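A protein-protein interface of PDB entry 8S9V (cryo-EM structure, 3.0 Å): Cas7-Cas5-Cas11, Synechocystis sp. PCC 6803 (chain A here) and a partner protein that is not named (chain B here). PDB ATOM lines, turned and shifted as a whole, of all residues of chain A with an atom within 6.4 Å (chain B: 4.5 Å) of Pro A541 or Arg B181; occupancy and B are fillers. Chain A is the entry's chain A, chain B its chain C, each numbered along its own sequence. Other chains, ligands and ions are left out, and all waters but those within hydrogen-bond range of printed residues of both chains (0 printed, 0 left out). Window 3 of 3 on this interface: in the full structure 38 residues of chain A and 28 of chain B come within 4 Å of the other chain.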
ATOM      1  N   PHE A 492      -3.078   9.423 -28.159  1.00  0.00           N
ATOM      2  CA  PHE A 492      -2.835  10.367 -29.244  1.00  0.00           C
ATOM      3  C   PHE A 492      -1.441  10.983 -29.251  1.00  0.00           C
ATOM      4  O   PHE A 492      -1.204  11.915 -30.017  1.00  0.00           O
ATOM      5  CB  PHE A 492      -3.900  11.457 -29.254  1.00  0.00           C
ATOM      6  CG  PHE A 492      -5.242  10.970 -29.667  1.00  0.00           C
ATOM      7  CD1 PHE A 492      -5.535  10.832 -30.996  1.00  0.00           C
ATOM      8  CD2 PHE A 492      -6.194  10.636 -28.754  1.00  0.00           C
ATOM      9  CE1 PHE A 492      -6.740  10.393 -31.411  1.00  0.00           C
ATOM     10  CE2 PHE A 492      -7.415  10.192 -29.174  1.00  0.00           C
ATOM     11  CZ  PHE A 492      -7.680  10.072 -30.510  1.00  0.00           C
ATOM     12  N   ARG A 528      -5.331  20.689 -29.795  1.00  0.00           N
ATOM     13  CA  ARG A 528      -6.098  19.860 -28.883  1.00  0.00           C
ATOM     14  C   ARG A 528      -7.550  20.286 -28.934  1.00  0.00           C
ATOM     15  O   ARG A 528      -7.861  21.467 -28.782  1.00  0.00           O
ATOM     16  CB  ARG A 528      -5.553  19.955 -27.476  1.00  0.00           C
ATOM     17  CG  ARG A 528      -6.321  19.214 -26.460  1.00  0.00           C
ATOM     18  CD  ARG A 528      -5.496  19.196 -25.236  1.00  0.00           C
ATOM     19  NE  ARG A 528      -6.207  18.737 -24.066  1.00  0.00           N
ATOM     20  CZ  ARG A 528      -5.597  18.354 -22.959  1.00  0.00           C
ATOM     21  NH1 ARG A 528      -6.300  17.979 -21.908  1.00  0.00           N
ATOM     22  NH2 ARG A 528      -4.281  18.345 -22.917  1.00  0.00           N
ATOM     23  N   THR A 529      -8.428  19.314 -29.129  1.00  0.00           N
ATOM     24  CA  THR A 529      -9.860  19.536 -29.196  1.00  0.00           C
ATOM     25  C   THR A 529     -10.517  18.974 -27.949  1.00  0.00           C
ATOM     26  O   THR A 529     -10.374  17.787 -27.655  1.00  0.00           O
ATOM     27  CB  THR A 529     -10.429  18.875 -30.444  1.00  0.00           C
ATOM     28  OG1 THR A 529      -9.758  19.389 -31.596  1.00  0.00           O
ATOM     29  CG2 THR A 529     -11.898  19.176 -30.578  1.00  0.00           C
ATOM     30  N   GLU A 530     -11.236  19.826 -27.230  1.00  0.00           N
ATOM     31  CA  GLU A 530     -12.109  19.427 -26.139  1.00  0.00           C
ATOM     32  C   GLU A 530     -13.565  19.655 -26.508  1.00  0.00           C
ATOM     33  O   GLU A 530     -13.937  20.767 -26.883  1.00  0.00           O
ATOM     34  CB  GLU A 530     -11.763  20.202 -24.872  1.00  0.00           C
ATOM     35  CG  GLU A 530     -10.393  19.893 -24.316  1.00  0.00           C
ATOM     36  CD  GLU A 530     -10.323  18.488 -23.765  1.00  0.00           C
ATOM     37  OE1 GLU A 530     -11.379  17.833 -23.699  1.00  0.00           O
ATOM     38  OE2 GLU A 530      -9.228  18.036 -23.386  1.00  0.00           O
ATOM     39  N   SER A 531     -14.382  18.605 -26.410  1.00  0.00           N
ATOM     40  CA  SER A 531     -15.739  18.652 -26.928  1.00  0.00           C
ATOM     41  C   SER A 531     -16.658  17.750 -26.112  1.00  0.00           C
ATOM     42  O   SER A 531     -16.226  16.720 -25.602  1.00  0.00           O
ATOM     43  CB  SER A 531     -15.728  18.233 -28.380  1.00  0.00           C
ATOM     44  OG  SER A 531     -17.042  18.079 -28.830  1.00  0.00           O
ATOM     45  N   TRP A 532     -17.929  18.136 -25.988  1.00  0.00           N
ATOM     46  CA  TRP A 532     -18.938  17.253 -25.411  1.00  0.00           C
ATOM     47  C   TRP A 532     -19.347  16.168 -26.401  1.00  0.00           C
ATOM     48  O   TRP A 532     -19.124  16.275 -27.603  1.00  0.00           O
ATOM     49  CB  TRP A 532     -20.156  18.051 -24.975  1.00  0.00           C
ATOM     50  CG  TRP A 532     -20.965  17.473 -23.842  1.00  0.00           C
ATOM     51  CD1 TRP A 532     -22.169  16.868 -23.936  1.00  0.00           C
ATOM     52  CD2 TRP A 532     -20.653  17.506 -22.449  1.00  0.00           C
ATOM     53  NE1 TRP A 532     -22.619  16.499 -22.706  1.00  0.00           N
ATOM     54  CE2 TRP A 532     -21.700  16.886 -21.774  1.00  0.00           C
ATOM     55  CE3 TRP A 532     -19.586  17.998 -21.709  1.00  0.00           C
ATOM     56  CZ2 TRP A 532     -21.709  16.741 -20.404  1.00  0.00           C
ATOM     57  CZ3 TRP A 532     -19.604  17.850 -20.361  1.00  0.00           C
ATOM     58  CH2 TRP A 532     -20.656  17.237 -19.719  1.00  0.00           C
ATOM     59  N   TRP A 536     -23.746  10.685 -25.112  1.00  0.00           N
ATOM     60  CA  TRP A 536     -23.193  10.143 -23.879  1.00  0.00           C
ATOM     61  C   TRP A 536     -23.635  10.930 -22.671  1.00  0.00           C
ATOM     62  O   TRP A 536     -23.809  10.362 -21.594  1.00  0.00           O
ATOM     63  CB  TRP A 536     -21.680  10.186 -23.900  1.00  0.00           C
ATOM     64  CG  TRP A 536     -21.002   9.321 -24.827  1.00  0.00           C
ATOM     65  CD1 TRP A 536     -21.551   8.484 -25.706  1.00  0.00           C
ATOM     66  CD2 TRP A 536     -19.596   9.206 -24.973  1.00  0.00           C
ATOM     67  NE1 TRP A 536     -20.578   7.829 -26.408  1.00  0.00           N
ATOM     68  CE2 TRP A 536     -19.360   8.264 -25.970  1.00  0.00           C
ATOM     69  CE3 TRP A 536     -18.514   9.817 -24.356  1.00  0.00           C
ATOM     70  CZ2 TRP A 536     -18.096   7.918 -26.367  1.00  0.00           C
ATOM     71  CZ3 TRP A 536     -17.273   9.477 -24.744  1.00  0.00           C
ATOM     72  CH2 TRP A 536     -17.063   8.535 -25.740  1.00  0.00           C
ATOM     73  N   PRO A 539     -18.264  14.591 -21.638  1.00  0.00           N
ATOM     74  CA  PRO A 539     -17.345  15.075 -22.660  1.00  0.00           C
ATOM     75  C   PRO A 539     -16.678  13.944 -23.407  1.00  0.00           C
ATOM     76  O   PRO A 539     -16.479  12.860 -22.874  1.00  0.00           O
ATOM     77  CB  PRO A 539     -16.348  15.912 -21.861  1.00  0.00           C
ATOM     78  CG  PRO A 539     -16.402  15.385 -20.544  1.00  0.00           C
ATOM     79  CD  PRO A 539     -17.795  14.956 -20.300  1.00  0.00           C
ATOM     80  N   ARG A 540     -16.336  14.204 -24.663  1.00  0.00           N
ATOM     81  CA  ARG A 540     -15.530  13.270 -25.416  1.00  0.00           C
ATOM     82  C   ARG A 540     -14.165  13.116 -24.764  1.00  0.00           C
ATOM     83  O   ARG A 540     -13.691  14.016 -24.074  1.00  0.00           O
ATOM     84  CB  ARG A 540     -15.370  13.755 -26.847  1.00  0.00           C
ATOM     85  CG  ARG A 540     -16.616  13.744 -27.650  1.00  0.00           C
ATOM     86  CD  ARG A 540     -16.396  14.498 -28.935  1.00  0.00           C
ATOM     87  NE  ARG A 540     -15.741  13.801 -30.009  1.00  0.00           N
ATOM     88  CZ  ARG A 540     -15.541  14.343 -31.199  1.00  0.00           C
ATOM     89  NH1 ARG A 540     -15.122  13.623 -32.215  1.00  0.00           N
ATOM     90  NH2 ARG A 540     -15.845  15.604 -31.386  1.00  0.00           N
ATOM     91  N   PRO A 541     -13.509  11.986 -24.981  1.00  0.00           N
ATOM     92  CA  PRO A 541     -12.075  11.923 -24.739  1.00  0.00           C
ATOM     93  C   PRO A 541     -11.356  13.004 -25.517  1.00  0.00           C
ATOM     94  O   PRO A 541     -11.715  13.321 -26.646  1.00  0.00           O
ATOM     95  CB  PRO A 541     -11.707  10.528 -25.228  1.00  0.00           C
ATOM     96  CG  PRO A 541     -12.714  10.221 -26.202  1.00  0.00           C
ATOM     97  CD  PRO A 541     -13.976  10.786 -25.674  1.00  0.00           C
ATOM     98  N   SER A 542     -10.355  13.598 -24.883  1.00  0.00           N
ATOM     99  CA  SER A 542      -9.628  14.698 -25.488  1.00  0.00           C
ATOM    100  C   SER A 542      -8.851  14.206 -26.693  1.00  0.00           C
ATOM    101  O   SER A 542      -8.150  13.197 -26.616  1.00  0.00           O
ATOM    102  CB  SER A 542      -8.703  15.318 -24.463  1.00  0.00           C
ATOM    103  OG  SER A 542      -8.117  16.477 -24.973  1.00  0.00           O
ATOM    104  N   LEU A 543      -8.981  14.915 -27.808  1.00  0.00           N
ATOM    105  CA  LEU A 543      -8.389  14.547 -29.091  1.00  0.00           C
ATOM    106  C   LEU A 543      -7.230  15.482 -29.380  1.00  0.00           C
ATOM    107  O   LEU A 543      -7.414  16.697 -29.431  1.00  0.00           O
ATOM    108  CB  LEU A 543      -9.414  14.628 -30.215  1.00  0.00           C
ATOM    109  CG  LEU A 543     -10.728  13.888 -30.049  1.00  0.00           C
ATOM    110  CD1 LEU A 543     -11.554  14.167 -31.238  1.00  0.00           C
ATOM    111  CD2 LEU A 543     -10.464  12.422 -29.933  1.00  0.00           C
ATOM    112  N   ARG A 577     -11.181   9.255 -36.790  1.00  0.00           N
ATOM    113  CA  ARG A 577     -12.432  10.019 -36.888  1.00  0.00           C
ATOM    114  C   ARG A 577     -12.543  10.815 -38.177  1.00  0.00           C
ATOM    115  O   ARG A 577     -13.094  11.909 -38.203  1.00  0.00           O
ATOM    116  CB  ARG A 577     -12.714  10.899 -35.676  1.00  0.00           C
ATOM    117  CG  ARG A 577     -13.017  10.091 -34.458  1.00  0.00           C
ATOM    118  CD  ARG A 577     -13.158  10.887 -33.213  1.00  0.00           C
ATOM    119  NE  ARG A 577     -12.581  10.191 -32.087  1.00  0.00           N
ATOM    120  CZ  ARG A 577     -13.262   9.918 -30.990  1.00  0.00           C
ATOM    121  NH1 ARG A 577     -12.695   9.287 -29.983  1.00  0.00           N
ATOM    122  NH2 ARG A 577     -14.522  10.271 -30.909  1.00  0.00           N
ATOM    123  N   PHE B 179      -2.327  15.419 -19.417  1.00  0.00           N
ATOM    124  CA  PHE B 179      -3.615  15.712 -18.781  1.00  0.00           C
ATOM    125  C   PHE B 179      -4.793  15.537 -19.737  1.00  0.00           C
ATOM    126  O   PHE B 179      -5.724  16.342 -19.756  1.00  0.00           O
ATOM    127  CB  PHE B 179      -3.642  17.115 -18.178  1.00  0.00           C
ATOM    128  CG  PHE B 179      -2.469  17.428 -17.319  1.00  0.00           C
ATOM    129  CD1 PHE B 179      -2.341  16.857 -16.088  1.00  0.00           C
ATOM    130  CD2 PHE B 179      -1.511  18.316 -17.728  1.00  0.00           C
ATOM    131  CE1 PHE B 179      -1.279  17.140 -15.302  1.00  0.00           C
ATOM    132  CE2 PHE B 179      -0.450  18.599 -16.934  1.00  0.00           C
ATOM    133  CZ  PHE B 179      -0.336  18.011 -15.723  1.00  0.00           C
ATOM    134  N   LEU B 180      -4.768  14.462 -20.516  1.00  0.00           N
ATOM    135  CA  LEU B 180      -5.850  14.181 -21.448  1.00  0.00           C
ATOM    136  C   LEU B 180      -7.131  13.796 -20.725  1.00  0.00           C
ATOM    137  O   LEU B 180      -7.137  12.918 -19.862  1.00  0.00           O
ATOM    138  CB  LEU B 180      -5.452  13.096 -22.433  1.00  0.00           C
ATOM    139  CG  LEU B 180      -4.811  13.662 -23.688  1.00  0.00           C
ATOM    140  CD1 LEU B 180      -3.571  14.346 -23.339  1.00  0.00           C
ATOM    141  CD2 LEU B 180      -4.511  12.566 -24.636  1.00  0.00           C
ATOM    142  N   ARG B 181      -8.219  14.448 -21.108  1.00  0.00           N
ATOM    143  CA  ARG B 181      -9.547  14.171 -20.580  1.00  0.00           C
ATOM    144  C   ARG B 181     -10.013  12.748 -20.831  1.00  0.00           C
ATOM    145  O   ARG B 181      -9.955  12.252 -21.958  1.00  0.00           O
ATOM    146  CB  ARG B 181     -10.556  15.108 -21.200  1.00  0.00           C
ATOM    147  CG  ARG B 181     -11.920  14.810 -20.727  1.00  0.00           C
ATOM    148  CD  ARG B 181     -12.152  15.398 -19.411  1.00  0.00           C
ATOM    149  NE  ARG B 181     -12.248  16.827 -19.537  1.00  0.00           N
ATOM    150  CZ  ARG B 181     -13.211  17.530 -18.978  1.00  0.00           C
ATOM    151  NH1 ARG B 181     -13.353  18.807 -19.250  1.00  0.00           N
ATOM    152  NH2 ARG B 181     -14.102  16.915 -18.234  1.00  0.00           N
ATOM    153  N   LEU B 182     -10.444  12.071 -19.750  1.00  0.00           N
ATOM    154  CA  LEU B 182     -11.382  10.964 -19.833  1.00  0.00           C
ATOM    155  C   LEU B 182     -12.801  11.492 -19.704  1.00  0.00           C
ATOM    156  O   LEU B 182     -13.027  12.508 -19.057  1.00  0.00           O
ATOM    157  CB  LEU B 182     -11.134   9.962 -18.727  1.00  0.00           C
ATOM    158  CG  LEU B 182      -9.883   9.124 -18.829  1.00  0.00           C
ATOM    159  CD1 LEU B 182      -9.049   9.435 -17.646  1.00  0.00           C
ATOM    160  CD2 LEU B 182     -10.269   7.682 -18.824  1.00  0.00           C
ATOM    161  N   PRO B 183     -13.786  10.860 -20.317  1.00  0.00           N
ATOM    162  CA  PRO B 183     -15.138  11.418 -20.263  1.00  0.00           C
ATOM    163  C   PRO B 183     -15.638  11.668 -18.860  1.00  0.00           C
ATOM    164  O   PRO B 183     -16.352  12.641 -18.627  1.00  0.00           O
ATOM    165  CB  PRO B 183     -15.958  10.333 -20.948  1.00  0.00           C
ATOM    166  CG  PRO B 183     -15.038   9.739 -21.877  1.00  0.00           C
ATOM    167  CD  PRO B 183     -13.740   9.671 -21.170  1.00  0.00           C
ATOM    168  N   ALA B 185     -14.146  12.635 -16.068  1.00  0.00           N
ATOM    169  CA  ALA B 185     -13.377  13.507 -15.194  1.00  0.00           C
ATOM    170  C   ALA B 185     -13.888  14.937 -15.270  1.00  0.00           C
ATOM    171  O   ALA B 185     -14.091  15.468 -16.358  1.00  0.00           O
ATOM    172  CB  ALA B 185     -11.905  13.458 -15.583  1.00  0.00           C
ATOM    173  N   ALA B 186     -14.053  15.566 -14.111  1.00  0.00           N
ATOM    174  CA  ALA B 186     -14.614  16.901 -13.996  1.00  0.00           C
ATOM    175  C   ALA B 186     -13.682  17.952 -14.579  1.00  0.00           C
ATOM    176  O   ALA B 186     -12.530  17.680 -14.900  1.00  0.00           O
ATOM    177  CB  ALA B 186     -14.928  17.217 -12.543  1.00  0.00           C
ATOM    178  N   GLY B 187     -14.214  19.169 -14.757  1.00  0.00           N
ATOM    179  CA  GLY B 187     -13.490  20.264 -15.367  1.00  0.00           C
ATOM    180  C   GLY B 187     -12.833  21.238 -14.395  1.00  0.00           C
ATOM    181  O   GLY B 187     -13.202  21.332 -13.236  1.00  0.00           O
ATOM    182  N   GLU B 192      -9.720  24.306 -19.924  1.00  0.00           N
ATOM    183  CA  GLU B 192     -10.267  23.130 -20.579  1.00  0.00           C
ATOM    184  C   GLU B 192      -9.751  21.821 -19.995  1.00  0.00           C
ATOM    185  O   GLU B 192     -10.299  20.771 -20.324  1.00  0.00           O
ATOM    186  CB  GLU B 192     -10.003  23.200 -22.080  1.00  0.00           C
ATOM    187  CG  GLU B 192      -8.601  22.853 -22.518  1.00  0.00           C
ATOM    188  CD  GLU B 192      -7.622  23.969 -22.238  1.00  0.00           C
ATOM    189  OE1 GLU B 192      -8.086  25.092 -21.953  1.00  0.00           O
ATOM    190  OE2 GLU B 192      -6.397  23.735 -22.334  1.00  0.00           O
ATOM    191  N   PRO B 194      -8.925  18.681 -17.414  1.00  0.00           N
ATOM    192  CA  PRO B 194      -9.691  18.027 -16.358  1.00  0.00           C
ATOM    193  C   PRO B 194      -9.207  18.417 -14.977  1.00  0.00           C
ATOM    194  O   PRO B 194      -8.009  18.520 -14.728  1.00  0.00           O
ATOM    195  CB  PRO B 194      -9.451  16.547 -16.629  1.00  0.00           C
ATOM    196  CG  PRO B 194      -8.179  16.508 -17.255  1.00  0.00           C
ATOM    197  CD  PRO B 194      -8.076  17.717 -18.113  1.00  0.00           C
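The backbone carbonyl oxygen of Phe B179 lies within hydrogen-bond range of the guanidinium group of Arg A528. The backbone carbonyl oxygen (O) of Arg B181 lies within hydrogen-bond range of the backbone NH (N) of Ser A542 (3.2 Å).
NE of Arg A528 is in salt-bridge range of OE2 of Glu A530, at 3.2 Å. NE of Arg A528 sits at hydrogen-bond distance from OG of Ser A542 (3.1 Å). OE2 of Glu A530 lies within hydrogen-bond range of OG of Ser A542 (2.5 Å). The backbone NH of Arg A540 sits at hydrogen-bond distance from the backbone carbonyl oxygen of Ser A531 (2.7 Å).
Among the printed residues, pairs that only touch across the chains: Pro A539 with Pro B183 (3.2 Å), Pro A541 with Arg B181 (3.5 Å), Pro A539 with Arg B181 (3.6 Å), Trp A536 with Pro B183 (3.6 Å), Glu A530 with Arg B181 (3.8 Å), Arg A528 with Leu B180 (3.9 Å), Arg A540 with Arg B181 (3.9 Å) and Glu A530 with Glu B192 (3.9 Å).
Of the printed residues of chain B, Arg A528 touches Phe B179 and Leu B180. Of the printed residues of chain B, Pro A539 touches Arg B181 (3.6 Å) and Pro B183 (3.2 Å). Of the printed residues of chain A, Arg B181 touches Glu A530 (3.8 Å), Pro A539 (3.6 Å), Arg A540 (3.9 Å), Pro A541 (3.5 Å) and Ser A542 (3.2 Å). The nearest residue of chain A that does not touch Arg B181 is Arg A528 (4.1 Å).
Printed residues of chain A that touch a printed residue of chain B: Arg A528, Glu A530, Trp A536, Pro A539, Arg A540, Pro A541 and Ser A542. Of the 10 printed residues of chain B, 5 touch a printed residue of chain A. Hydrophobic or aromatic side chains of chain B that line the printed part of chain A: Pro B183.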
